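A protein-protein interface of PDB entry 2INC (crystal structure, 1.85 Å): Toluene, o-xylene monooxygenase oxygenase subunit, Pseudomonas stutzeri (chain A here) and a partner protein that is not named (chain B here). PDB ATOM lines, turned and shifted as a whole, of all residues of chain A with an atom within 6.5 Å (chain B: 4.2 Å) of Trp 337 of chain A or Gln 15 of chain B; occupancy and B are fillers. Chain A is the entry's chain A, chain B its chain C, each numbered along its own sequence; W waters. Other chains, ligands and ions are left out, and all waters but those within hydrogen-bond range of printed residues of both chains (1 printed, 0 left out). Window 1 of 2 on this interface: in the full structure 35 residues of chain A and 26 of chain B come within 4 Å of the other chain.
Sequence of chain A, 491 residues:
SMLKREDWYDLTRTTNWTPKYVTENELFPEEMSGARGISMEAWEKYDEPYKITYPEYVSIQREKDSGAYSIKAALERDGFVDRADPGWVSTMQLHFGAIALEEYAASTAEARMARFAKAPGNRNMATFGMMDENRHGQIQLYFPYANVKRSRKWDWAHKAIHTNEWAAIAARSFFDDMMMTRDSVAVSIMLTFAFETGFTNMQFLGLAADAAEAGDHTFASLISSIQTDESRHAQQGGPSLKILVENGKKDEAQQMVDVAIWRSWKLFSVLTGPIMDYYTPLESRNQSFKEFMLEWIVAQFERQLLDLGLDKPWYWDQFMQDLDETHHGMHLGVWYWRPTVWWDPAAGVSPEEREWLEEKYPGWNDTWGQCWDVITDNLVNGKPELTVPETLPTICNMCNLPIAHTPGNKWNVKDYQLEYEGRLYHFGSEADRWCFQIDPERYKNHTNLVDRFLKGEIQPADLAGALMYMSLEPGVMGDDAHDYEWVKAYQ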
ATOM      1  N   TRP A 166      -6.428  12.831 -13.997  1.00  0.00           N
ATOM      2  CA  TRP A 166      -6.249  11.377 -13.959  1.00  0.00           C
ATOM      3  C   TRP A 166      -7.124  10.649 -14.993  1.00  0.00           C
ATOM      4  O   TRP A 166      -6.728   9.598 -15.508  1.00  0.00           O
ATOM      5  CB  TRP A 166      -6.521  10.793 -12.541  1.00  0.00           C
ATOM      6  CG  TRP A 166      -7.948  10.966 -12.118  1.00  0.00           C
ATOM      7  CD1 TRP A 166      -8.485  12.037 -11.490  1.00  0.00           C
ATOM      8  CD2 TRP A 166      -9.025  10.066 -12.377  1.00  0.00           C
ATOM      9  NE1 TRP A 166      -9.845  11.878 -11.323  1.00  0.00           N
ATOM     10  CE2 TRP A 166     -10.196  10.655 -11.845  1.00  0.00           C
ATOM     11  CE3 TRP A 166      -9.114   8.793 -12.985  1.00  0.00           C
ATOM     12  CZ2 TRP A 166     -11.437  10.048 -11.936  1.00  0.00           C
ATOM     13  CZ3 TRP A 166     -10.346   8.206 -13.095  1.00  0.00           C
ATOM     14  CH2 TRP A 166     -11.495   8.818 -12.557  1.00  0.00           C
ATOM     15  N   LEU A 332     -18.565   5.539  -7.397  1.00  0.00           N
ATOM     16  CA  LEU A 332     -18.356   6.034  -6.034  1.00  0.00           C
ATOM     17  C   LEU A 332     -17.005   6.749  -5.944  1.00  0.00           C
ATOM     18  O   LEU A 332     -16.897   7.847  -5.314  1.00  0.00           O
ATOM     19  CB  LEU A 332     -18.445   4.859  -5.044  1.00  0.00           C
ATOM     20  CG  LEU A 332     -18.189   5.175  -3.546  1.00  0.00           C
ATOM     21  CD1 LEU A 332     -18.749   6.516  -3.094  1.00  0.00           C
ATOM     22  CD2 LEU A 332     -18.652   4.086  -2.628  1.00  0.00           C
ATOM     23  N   GLY A 333     -15.993   6.182  -6.617  1.00  0.00           N
ATOM     24  CA  GLY A 333     -14.687   6.825  -6.675  1.00  0.00           C
ATOM     25  C   GLY A 333     -14.745   8.203  -7.328  1.00  0.00           C
ATOM     26  O   GLY A 333     -14.205   9.173  -6.787  1.00  0.00           O
ATOM     27  N   VAL A 334     -15.352   8.279  -8.518  1.00  0.00           N
ATOM     28  CA  VAL A 334     -15.500   9.562  -9.180  1.00  0.00           C
ATOM     29  C   VAL A 334     -16.328  10.573  -8.377  1.00  0.00           C
ATOM     30  O   VAL A 334     -15.988  11.776  -8.367  1.00  0.00           O
ATOM     31  CB  VAL A 334     -16.042   9.431 -10.674  1.00  0.00           C
ATOM     32  CG1 VAL A 334     -16.340  10.836 -11.253  1.00  0.00           C
ATOM     33  CG2 VAL A 334     -15.045   8.732 -11.571  1.00  0.00           C
ATOM     34  N   TRP A 335     -17.448  10.145  -7.767  1.00  0.00           N
ATOM     35  CA  TRP A 335     -18.244  11.107  -6.970  1.00  0.00           C
ATOM     36  C   TRP A 335     -17.415  11.533  -5.737  1.00  0.00           C
ATOM     37  O   TRP A 335     -17.338  12.756  -5.408  1.00  0.00           O
ATOM     38  CB  TRP A 335     -19.625  10.521  -6.517  1.00  0.00           C
ATOM     39  CG  TRP A 335     -20.491  11.588  -5.896  1.00  0.00           C
ATOM     40  CD1 TRP A 335     -21.338  12.439  -6.529  1.00  0.00           C
ATOM     41  CD2 TRP A 335     -20.519  11.964  -4.509  1.00  0.00           C
ATOM     42  NE1 TRP A 335     -21.918  13.310  -5.634  1.00  0.00           N
ATOM     43  CE2 TRP A 335     -21.422  13.049  -4.385  1.00  0.00           C
ATOM     44  CE3 TRP A 335     -19.860  11.492  -3.369  1.00  0.00           C
ATOM     45  CZ2 TRP A 335     -21.719  13.642  -3.150  1.00  0.00           C
ATOM     46  CZ3 TRP A 335     -20.141  12.090  -2.140  1.00  0.00           C
ATOM     47  CH2 TRP A 335     -21.050  13.167  -2.051  1.00  0.00           C
ATOM     48  N   TYR A 336     -16.804  10.557  -5.071  1.00  0.00           N
ATOM     49  CA  TYR A 336     -16.087  10.921  -3.841  1.00  0.00           C
ATOM     50  C   TYR A 336     -14.937  11.880  -4.190  1.00  0.00           C
ATOM     51  O   TYR A 336     -14.770  12.904  -3.526  1.00  0.00           O
ATOM     52  CB  TYR A 336     -15.608   9.710  -3.024  1.00  0.00           C
ATOM     53  CG  TYR A 336     -15.303  10.088  -1.575  1.00  0.00           C
ATOM     54  CD1 TYR A 336     -16.305  10.028  -0.591  1.00  0.00           C
ATOM     55  CD2 TYR A 336     -14.039  10.521  -1.196  1.00  0.00           C
ATOM     56  CE1 TYR A 336     -16.048  10.378   0.755  1.00  0.00           C
ATOM     57  CE2 TYR A 336     -13.776  10.889   0.155  1.00  0.00           C
ATOM     58  CZ  TYR A 336     -14.786  10.804   1.108  1.00  0.00           C
ATOM     59  OH  TYR A 336     -14.548  11.133   2.436  1.00  0.00           O
ATOM     60  N   TRP A 337     -14.184  11.581  -5.266  1.00  0.00           N
ATOM     61  CA  TRP A 337     -13.108  12.435  -5.715  1.00  0.00           C
ATOM     62  C   TRP A 337     -13.531  13.475  -6.762  1.00  0.00           C
ATOM     63  O   TRP A 337     -12.715  13.891  -7.591  1.00  0.00           O
ATOM     64  CB  TRP A 337     -11.933  11.608  -6.253  1.00  0.00           C
ATOM     65  CG  TRP A 337     -11.003  11.179  -5.166  1.00  0.00           C
ATOM     66  CD1 TRP A 337      -9.869  11.842  -4.736  1.00  0.00           C
ATOM     67  CD2 TRP A 337     -11.128  10.029  -4.338  1.00  0.00           C
ATOM     68  NE1 TRP A 337      -9.280  11.165  -3.702  1.00  0.00           N
ATOM     69  CE2 TRP A 337     -10.021  10.039  -3.436  1.00  0.00           C
ATOM     70  CE3 TRP A 337     -12.065   8.987  -4.255  1.00  0.00           C
ATOM     71  CZ2 TRP A 337      -9.835   9.045  -2.453  1.00  0.00           C
ATOM     72  CZ3 TRP A 337     -11.877   7.988  -3.277  1.00  0.00           C
ATOM     73  CH2 TRP A 337     -10.751   8.037  -2.387  1.00  0.00           C
ATOM     74  N   ARG A 338     -14.785  13.915  -6.688  1.00  0.00           N
ATOM     75  CA  ARG A 338     -15.366  14.836  -7.665  1.00  0.00           C
ATOM     76  C   ARG A 338     -14.627  16.134  -7.994  1.00  0.00           C
ATOM     77  O   ARG A 338     -14.754  16.608  -9.121  1.00  0.00           O
ATOM     78  CB  ARG A 338     -16.854  15.158  -7.345  1.00  0.00           C
ATOM     79  CG  ARG A 338     -17.134  15.742  -5.904  1.00  0.00           C
ATOM     80  CD  ARG A 338     -18.631  15.679  -5.548  1.00  0.00           C
ATOM     81  NE  ARG A 338     -18.861  16.248  -4.203  1.00  0.00           N
ATOM     82  CZ  ARG A 338     -18.566  15.610  -3.073  1.00  0.00           C
ATOM     83  NH1 ARG A 338     -18.844  16.198  -1.914  1.00  0.00           N
ATOM     84  NH2 ARG A 338     -18.032  14.375  -3.090  1.00  0.00           N
ATOM     85  N   PRO A 339     -13.892  16.751  -7.035  1.00  0.00           N
ATOM     86  CA  PRO A 339     -13.157  17.948  -7.491  1.00  0.00           C
ATOM     87  C   PRO A 339     -12.011  17.619  -8.475  1.00  0.00           C
ATOM     88  O   PRO A 339     -11.420  18.538  -9.058  1.00  0.00           O
ATOM     89  CB  PRO A 339     -12.567  18.537  -6.195  1.00  0.00           C
ATOM     90  CG  PRO A 339     -13.334  17.916  -5.063  1.00  0.00           C
ATOM     91  CD  PRO A 339     -13.684  16.502  -5.592  1.00  0.00           C
ATOM     92  N   THR A 340     -11.705  16.338  -8.632  1.00  0.00           N
ATOM     93  CA  THR A 340     -10.624  15.927  -9.522  1.00  0.00           C
ATOM     94  C   THR A 340     -11.070  15.591 -10.948  1.00  0.00           C
ATOM     95  O   THR A 340     -10.224  15.089 -11.742  1.00  0.00           O
ATOM     96  CB  THR A 340      -9.866  14.708  -9.021  1.00  0.00           C
ATOM     97  OG1 THR A 340     -10.672  13.542  -9.214  1.00  0.00           O
ATOM     98  CG2 THR A 340      -9.458  14.862  -7.520  1.00  0.00           C
ATOM     99  N   VAL A 341     -12.332  15.865 -11.288  1.00  0.00           N
ATOM    100  CA  VAL A 341     -12.787  15.738 -12.674  1.00  0.00           C
ATOM    101  C   VAL A 341     -13.358  17.050 -13.160  1.00  0.00           C
ATOM    102  O   VAL A 341     -13.580  17.969 -12.375  1.00  0.00           O
ATOM    103  CB  VAL A 341     -13.833  14.626 -12.854  1.00  0.00           C
ATOM    104  CG1 VAL A 341     -13.249  13.250 -12.476  1.00  0.00           C
ATOM    105  CG2 VAL A 341     -15.066  14.924 -12.021  1.00  0.00           C
ATOM    106  N   PRO A 345     -20.195  14.991 -11.118  1.00  0.00           N
ATOM    107  CA  PRO A 345     -20.845  13.685 -10.976  1.00  0.00           C
ATOM    108  C   PRO A 345     -22.205  13.741 -10.217  1.00  0.00           C
ATOM    109  O   PRO A 345     -22.359  14.490  -9.236  1.00  0.00           O
ATOM    110  CB  PRO A 345     -19.839  12.847 -10.174  1.00  0.00           C
ATOM    111  CG  PRO A 345     -18.561  13.568 -10.235  1.00  0.00           C
ATOM    112  CD  PRO A 345     -18.905  15.046 -10.398  1.00  0.00           C
ATOM    113  N   THR A 387     -17.152  14.264   3.050  1.00  0.00           N
ATOM    114  CA  THR A 387     -17.604  13.651   1.765  1.00  0.00           C
ATOM    115  C   THR A 387     -16.643  13.952   0.588  1.00  0.00           C
ATOM    116  O   THR A 387     -16.915  13.595  -0.555  1.00  0.00           O
ATOM    117  CB  THR A 387     -19.053  14.055   1.393  1.00  0.00           C
ATOM    118  OG1 THR A 387     -19.057  15.414   0.944  1.00  0.00           O
ATOM    119  CG2 THR A 387     -19.980  13.936   2.622  1.00  0.00           C
ATOM    120  N   VAL A 388     -15.537  14.631   0.885  1.00  0.00           N
ATOM    121  CA  VAL A 388     -14.451  14.873  -0.073  1.00  0.00           C
ATOM    122  C   VAL A 388     -13.175  14.395   0.555  1.00  0.00           C
ATOM    123  O   VAL A 388     -13.052  14.444   1.771  1.00  0.00           O
ATOM    124  CB  VAL A 388     -14.297  16.358  -0.417  1.00  0.00           C
ATOM    125  CG1 VAL A 388     -15.450  16.816  -1.325  1.00  0.00           C
ATOM    126  CG2 VAL A 388     -14.210  17.223   0.838  1.00  0.00           C
ATOM    127  N   PRO A 389     -12.199  13.985  -0.268  1.00  0.00           N
ATOM    128  CA  PRO A 389     -11.026  13.262   0.233  1.00  0.00           C
ATOM    129  C   PRO A 389      -9.871  14.150   0.611  1.00  0.00           C
ATOM    130  O   PRO A 389      -9.763  15.315   0.173  1.00  0.00           O
ATOM    131  CB  PRO A 389     -10.580  12.438  -0.977  1.00  0.00           C
ATOM    132  CG  PRO A 389     -10.864  13.400  -2.128  1.00  0.00           C
ATOM    133  CD  PRO A 389     -12.157  14.149  -1.743  1.00  0.00           C
ATOM    134  N   GLU A 390      -8.975  13.549   1.370  1.00  0.00           N
ATOM    135  CA  GLU A 390      -7.790  14.226   1.828  1.00  0.00           C
ATOM    136  C   GLU A 390      -6.573  13.383   1.463  1.00  0.00           C
ATOM    137  O   GLU A 390      -5.450  13.622   1.925  1.00  0.00           O
ATOM    138  CB  GLU A 390      -7.907  14.403   3.345  1.00  0.00           C
ATOM    139  CG  GLU A 390      -8.887  15.488   3.716  1.00  0.00           C
ATOM    140  CD  GLU A 390      -8.910  15.711   5.198  1.00  0.00           C
ATOM    141  OE1 GLU A 390      -7.811  15.843   5.791  1.00  0.00           O
ATOM    142  OE2 GLU A 390     -10.031  15.721   5.781  1.00  0.00           O
ATOM    143  N   THR A 391      -6.805  12.367   0.650  1.00  0.00           N
ATOM    144  CA  THR A 391      -5.727  11.615   0.056  1.00  0.00           C
ATOM    145  C   THR A 391      -6.054  11.136  -1.386  1.00  0.00           C
ATOM    146  O   THR A 391      -7.156  11.393  -1.877  1.00  0.00           O
ATOM    147  CB  THR A 391      -5.321  10.470   0.945  1.00  0.00           C
ATOM    148  OG1 THR A 391      -4.037  10.012   0.506  1.00  0.00           O
ATOM    149  CG2 THR A 391      -6.397   9.317   0.954  1.00  0.00           C
ATOM    150  N   LEU A 392      -5.098  10.458  -2.017  1.00  0.00           N
ATOM    151  CA  LEU A 392      -5.229   9.973  -3.372  1.00  0.00           C
ATOM    152  C   LEU A 392      -5.646   8.511  -3.231  1.00  0.00           C
ATOM    153  O   LEU A 392      -5.175   7.810  -2.320  1.00  0.00           O
ATOM    154  CB  LEU A 392      -3.880   9.996  -4.148  1.00  0.00           C
ATOM    155  CG  LEU A 392      -2.827  11.091  -4.413  1.00  0.00           C
ATOM    156  CD1 LEU A 392      -2.484  11.257  -5.896  1.00  0.00           C
ATOM    157  CD2 LEU A 392      -3.174  12.455  -3.872  1.00  0.00           C
ATOM    158  N   PRO A 393      -6.488   8.026  -4.157  1.00  0.00           N
ATOM    159  CA  PRO A 393      -6.676   6.581  -4.165  1.00  0.00           C
ATOM    160  C   PRO A 393      -5.471   5.889  -4.775  1.00  0.00           C
ATOM    161  O   PRO A 393      -4.713   6.504  -5.512  1.00  0.00           O
ATOM    162  CB  PRO A 393      -7.889   6.397  -5.063  1.00  0.00           C
ATOM    163  CG  PRO A 393      -7.732   7.509  -6.092  1.00  0.00           C
ATOM    164  CD  PRO A 393      -7.239   8.694  -5.243  1.00  0.00           C
ATOM    165  N   THR A 394      -5.303   4.597  -4.505  1.00  0.00           N
ATOM    166  CA  THR A 394      -4.319   3.823  -5.219  1.00  0.00           C
ATOM    167  C   THR A 394      -4.748   3.663  -6.695  1.00  0.00           C
ATOM    168  O   THR A 394      -5.877   3.262  -6.995  1.00  0.00           O
ATOM    169  CB  THR A 394      -4.207   2.456  -4.586  1.00  0.00           C
ATOM    170  OG1 THR A 394      -3.903   2.662  -3.196  1.00  0.00           O
ATOM    171  CG2 THR A 394      -3.094   1.655  -5.209  1.00  0.00           C
ATOM    172  N   ILE A 403      -8.171   1.358  -7.675  1.00  0.00           N
ATOM    173  CA  ILE A 403      -8.423  -0.048  -7.386  1.00  0.00           C
ATOM    174  C   ILE A 403      -9.564  -0.051  -6.363  1.00  0.00           C
ATOM    175  O   ILE A 403      -9.401   0.449  -5.260  1.00  0.00           O
ATOM    176  CB  ILE A 403      -7.186  -0.701  -6.831  1.00  0.00           C
ATOM    177  CG1 ILE A 403      -6.039  -0.640  -7.872  1.00  0.00           C
ATOM    178  CG2 ILE A 403      -7.504  -2.152  -6.382  1.00  0.00           C
ATOM    179  CD1 ILE A 403      -4.746  -1.393  -7.432  1.00  0.00           C
ATOM    180  N   LEU A 463      -2.620  18.143  -1.799  1.00  0.00           N
ATOM    181  CA  LEU A 463      -3.775  17.936  -2.646  1.00  0.00           C
ATOM    182  C   LEU A 463      -3.969  19.122  -3.587  1.00  0.00           C
ATOM    183  O   LEU A 463      -4.315  18.939  -4.760  1.00  0.00           O
ATOM    184  CB  LEU A 463      -5.026  17.732  -1.761  1.00  0.00           C
ATOM    185  CG  LEU A 463      -5.230  16.325  -1.164  1.00  0.00           C
ATOM    186  CD1 LEU A 463      -6.728  16.012  -1.269  1.00  0.00           C
ATOM    187  CD2 LEU A 463      -4.473  15.216  -1.834  1.00  0.00           C
ATOM    188  N   GLY A 478     -15.040  19.314 -10.231  1.00  0.00           N
ATOM    189  CA  GLY A 478     -16.400  18.846 -10.155  1.00  0.00           C
ATOM    190  C   GLY A 478     -16.994  18.959  -8.748  1.00  0.00           C
ATOM    191  O   GLY A 478     -16.272  19.073  -7.763  1.00  0.00           O
ATOM    192  N   ILE B   4       2.303   3.753   2.439  1.00  0.00           N
ATOM    193  CA  ILE B   4       1.636   2.486   2.273  1.00  0.00           C
ATOM    194  C   ILE B   4       0.283   2.710   1.592  1.00  0.00           C
ATOM    195  O   ILE B   4      -0.229   3.851   1.525  1.00  0.00           O
ATOM    196  CB  ILE B   4       1.463   1.696   3.630  1.00  0.00           C
ATOM    197  CG1 ILE B   4       0.693   2.518   4.657  1.00  0.00           C
ATOM    198  CG2 ILE B   4       2.844   1.239   4.195  1.00  0.00           C
ATOM    199  CD1 ILE B   4      -0.754   2.206   4.756  1.00  0.00           C
ATOM    200  N   MET B   5      -0.293   1.608   1.124  1.00  0.00           N
ATOM    201  CA  MET B   5      -1.650   1.557   0.540  1.00  0.00           C
ATOM    202  C   MET B   5      -2.605   0.832   1.497  1.00  0.00           C
ATOM    203  O   MET B   5      -2.417  -0.345   1.849  1.00  0.00           O
ATOM    204  CB  MET B   5      -1.657   0.830  -0.849  1.00  0.00           C
ATOM    205  CG  MET B   5      -0.692   1.443  -1.915  1.00  0.00           C
ATOM    206  SD  MET B   5      -0.943   3.204  -2.163  1.00  0.00           S
ATOM    207  CE  MET B   5       0.076   3.512  -3.614  1.00  0.00           C
ATOM    208  N   SER B   6      -3.649   1.535   1.883  1.00  0.00           N
ATOM    209  CA  SER B   6      -4.571   1.078   2.905  1.00  0.00           C
ATOM    210  C   SER B   6      -5.792   0.508   2.255  1.00  0.00           C
ATOM    211  O   SER B   6      -6.479   1.237   1.562  1.00  0.00           O
ATOM    212  CB  SER B   6      -4.984   2.310   3.726  1.00  0.00           C
ATOM    213  OG  SER B   6      -6.101   2.011   4.554  1.00  0.00           O
ATOM    214  N   ASP B  11     -14.537  -0.688   3.428  1.00  0.00           N
ATOM    215  CA  ASP B  11     -14.400   0.370   2.414  1.00  0.00           C
ATOM    216  C   ASP B  11     -14.433  -0.252   0.983  1.00  0.00           C
ATOM    217  O   ASP B  11     -14.398  -1.490   0.819  1.00  0.00           O
ATOM    218  CB  ASP B  11     -13.117   1.169   2.629  1.00  0.00           C
ATOM    219  CG  ASP B  11     -13.252   2.637   2.182  1.00  0.00           C
ATOM    220  OD1 ASP B  11     -14.139   2.971   1.355  1.00  0.00           O
ATOM    221  OD2 ASP B  11     -12.457   3.480   2.650  1.00  0.00           O
ATOM    222  N   VAL B  13     -12.342   1.096  -1.637  1.00  0.00           N
ATOM    223  CA  VAL B  13     -11.191   1.600  -2.376  1.00  0.00           C
ATOM    224  C   VAL B  13      -9.914   1.496  -1.566  1.00  0.00           C
ATOM    225  O   VAL B  13      -9.927   1.706  -0.359  1.00  0.00           O
ATOM    226  CB  VAL B  13     -11.443   3.053  -2.818  1.00  0.00           C
ATOM    227  CG1 VAL B  13     -11.386   4.052  -1.638  1.00  0.00           C
ATOM    228  CG2 VAL B  13     -10.524   3.435  -3.968  1.00  0.00           C
ATOM    229  N   ILE B  14      -8.811   1.166  -2.235  1.00  0.00           N
ATOM    230  CA  ILE B  14      -7.474   1.209  -1.624  1.00  0.00           C
ATOM    231  C   ILE B  14      -6.948   2.645  -1.754  1.00  0.00           C
ATOM    232  O   ILE B  14      -7.223   3.352  -2.759  1.00  0.00           O
ATOM    233  CB  ILE B  14      -6.536   0.157  -2.257  1.00  0.00           C
ATOM    234  CG1 ILE B  14      -7.258  -1.229  -2.301  1.00  0.00           C
ATOM    235  CG2 ILE B  14      -5.230   0.106  -1.525  1.00  0.00           C
ATOM    236  CD1 ILE B  14      -6.372  -2.437  -2.712  1.00  0.00           C
ATOM    237  N   GLN B  15      -6.289   3.124  -0.697  1.00  0.00           N
ATOM    238  CA  GLN B  15      -5.904   4.525  -0.660  1.00  0.00           C
ATOM    239  C   GLN B  15      -4.468   4.661  -0.240  1.00  0.00           C
ATOM    240  O   GLN B  15      -3.941   3.794   0.500  1.00  0.00           O
ATOM    241  CB  GLN B  15      -6.757   5.292   0.333  1.00  0.00           C
ATOM    242  CG  GLN B  15      -8.213   5.269   0.018  1.00  0.00           C
ATOM    243  CD  GLN B  15      -8.994   5.913   1.094  1.00  0.00           C
ATOM    244  OE1 GLN B  15      -9.303   5.269   2.122  1.00  0.00           O
ATOM    245  NE2 GLN B  15      -9.312   7.217   0.907  1.00  0.00           N
ATOM    246  N   LEU B  16      -3.839   5.753  -0.687  1.00  0.00           N
ATOM    247  CA  LEU B  16      -2.471   6.039  -0.265  1.00  0.00           C
ATOM    248  C   LEU B  16      -2.510   6.714   1.130  1.00  0.00           C
ATOM    249  O   LEU B  16      -3.209   7.703   1.315  1.00  0.00           O
ATOM    250  CB  LEU B  16      -1.773   6.940  -1.282  1.00  0.00           C
ATOM    251  CG  LEU B  16      -0.414   7.565  -0.871  1.00  0.00           C
ATOM    252  CD1 LEU B  16       0.716   6.505  -0.748  1.00  0.00           C
ATOM    253  CD2 LEU B  16      -0.020   8.643  -1.846  1.00  0.00           C
ATOM    254  N   VAL B  17      -1.751   6.182   2.077  1.00  0.00           N
ATOM    255  CA  VAL B  17      -1.706   6.717   3.447  1.00  0.00           C
ATOM    256  C   VAL B  17      -0.222   6.747   3.849  1.00  0.00           C
ATOM    257  O   VAL B  17       0.412   5.689   3.962  1.00  0.00           O
ATOM    258  CB  VAL B  17      -2.507   5.835   4.426  1.00  0.00           C
ATOM    259  CG1 VAL B  17      -2.391   6.352   5.845  1.00  0.00           C
ATOM    260  CG2 VAL B  17      -3.968   5.796   4.041  1.00  0.00           C
ATOM    261  N   HIS B  35      -9.085   8.022   6.924  1.00  0.00           N
ATOM    262  CA  HIS B  35      -9.488   8.172   5.523  1.00  0.00           C
ATOM    263  C   HIS B  35     -10.665   7.272   5.174  1.00  0.00           C
ATOM    264  O   HIS B  35     -11.083   7.242   4.007  1.00  0.00           O
ATOM    265  CB  HIS B  35      -8.302   7.903   4.588  1.00  0.00           C
ATOM    266  CG  HIS B  35      -7.227   8.938   4.684  1.00  0.00           C
ATOM    267  ND1 HIS B  35      -7.391  10.236   4.236  1.00  0.00           N
ATOM    268  CD2 HIS B  35      -5.984   8.881   5.220  1.00  0.00           C
ATOM    269  CE1 HIS B  35      -6.296  10.932   4.496  1.00  0.00           C
ATOM    270  NE2 HIS B  35      -5.428  10.134   5.092  1.00  0.00           N
ATOM    271  N   SER B  36     -11.225   6.565   6.162  1.00  0.00           N
ATOM    272  CA  SER B  36     -12.299   5.593   5.904  1.00  0.00           C
ATOM    273  C   SER B  36     -13.427   5.628   6.929  1.00  0.00           C
ATOM    274  O   SER B  36     -14.596   5.750   6.546  1.00  0.00           O
ATOM    275  CB  SER B  36     -11.739   4.188   5.829  1.00  0.00           C
ATOM    276  OG  SER B  36     -10.736   4.109   4.805  1.00  0.00           O
ATOM    277  N   ARG B  40     -16.925   6.845   4.565  1.00  0.00           N
ATOM    278  CA  ARG B  40     -17.420   5.666   4.212  1.00  0.00           C
ATOM    279  C   ARG B  40     -17.503   4.373   5.014  1.00  0.00           C
ATOM    280  O   ARG B  40     -18.007   3.513   4.474  1.00  0.00           O
ATOM    281  CB  ARG B  40     -16.764   5.321   2.970  1.00  0.00           C
ATOM    282  CG  ARG B  40     -16.810   6.261   2.028  1.00  0.00           C
ATOM    283  CD  ARG B  40     -15.884   5.964   0.827  1.00  0.00           C
ATOM    284  NE  ARG B  40     -14.997   7.049   0.735  1.00  0.00           N
ATOM    285  CZ  ARG B  40     -13.738   7.075   0.938  1.00  0.00           C
ATOM    286  NH1 ARG B  40     -12.993   6.038   1.105  1.00  0.00           N
ATOM    287  NH2 ARG B  40     -13.298   8.159   0.773  1.00  0.00           N
HETATM  288  O   HOH W   1      -9.641  11.107   2.734  1.00  0.00           O
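The backbone carbonyl oxygen of Leu 392 of chain A sits at hydrogen-bond distance from the backbone NH of Leu 16 of chain B. OG1 of Thr 394 of chain A is in hydrogen-bond range of N of Gln 15 of chain B (3.5 Å). The backbone carbonyl oxygen (O) of Leu 16 of chain B lies within hydrogen-bond range of the side-chain hydroxyl (OG1) of Thr 391 of chain A (2.6 Å). The side-chain hydroxyl of Thr 394 of chain A lies within hydrogen-bond range of the side-chain sulfur of Met 5 of chain B. The backbone NH (N) of Ile 14 of chain B is in hydrogen-bond range of the backbone carbonyl oxygen (O) of Ile 403 of chain A, at 3.2 Å. The backbone NH of Thr 394 of chain A sits at hydrogen-bond distance from the backbone carbonyl oxygen of Ile 14 of chain B, at 2.9 Å.
N of Ser 6 of chain B sits at hydrogen-bond distance from O of Gln 15 of chain B (2.7 Å). The backbone carbonyl oxygen (O) of Thr 394 of chain A is in hydrogen-bond range of the backbone NH (N) of Ile 403 of chain A (3.1 Å). The indole nitrogen (NE1) of Trp 337 of chain A lies within hydrogen-bond range of the backbone carbonyl oxygen (O) of Thr 391 of chain A (2.8 Å). O of Trp 337 of chain A is in hydrogen-bond range of OG1 of Thr 340 of chain A (2.6 Å). OE1 of Gln 15 of chain B sits close to O of His 35 of chain B (3.3 Å). OD2 of Asp 11 of chain B lies within salt-bridge range of NH1 of Arg 40 of chain B, 3.0 Å away.
Among the printed residues, pairs that only touch across the chains: Tyr 336 of chain A with Arg 40 of chain B (2.8 Å), Trp 337 of chain A with Gln 15 of chain B (3.7 Å), Glu 390 of chain A with His 35 of chain B (3.8 Å), Thr 391 of chain A with Gln 15 of chain B (3.6 Å), Thr 391 of chain A with His 35 of chain B (3.6 Å), Leu 392 of chain A with Gln 15 of chain B (3.8 Å), Pro 393 of chain A with Ile 14 of chain B (3.6 Å), Thr 394 of chain A with Leu 16 of chain B (3.98 Å) and Ile 403 of chain A with Val 13 of chain B (3.4 Å).
Printed residues of chain B within 4 Å of Tyr 336 of chain A: Arg 40. Of the printed residues of chain B, Trp 337 of chain A touches Gln 15. Of the printed residues of chain B, Ile 403 of chain A touches Val 13 and Ile 14. Of the printed residues of chain A, Gln 15 of chain B touches Trp 337 (3.7 Å), Thr 391 (3.6 Å), Leu 392 (3.8 Å) and Thr 394 (3.5 Å). The nearest residue of chain B that does not touch Trp 337 of chain A is Arg 40 of chain B (4.1 Å). The nearest residue of chain A that does not touch Gln 15 of chain B is Pro 393 of chain A (4.1 Å).
Printed residues of chain B that touch a printed residue of chain A: Met 5, Val 13, Ile 14, Gln 15, Leu 16, His 35 and Arg 40. Of the 23 printed residues of chain A, 8 touch a printed residue of chain B. Among the printed residues, 15 pairs touch across the chains.
Water W1 lies within hydrogen-bond range of ND1 of His 35 of chain B and N of Glu 390 of chain A.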
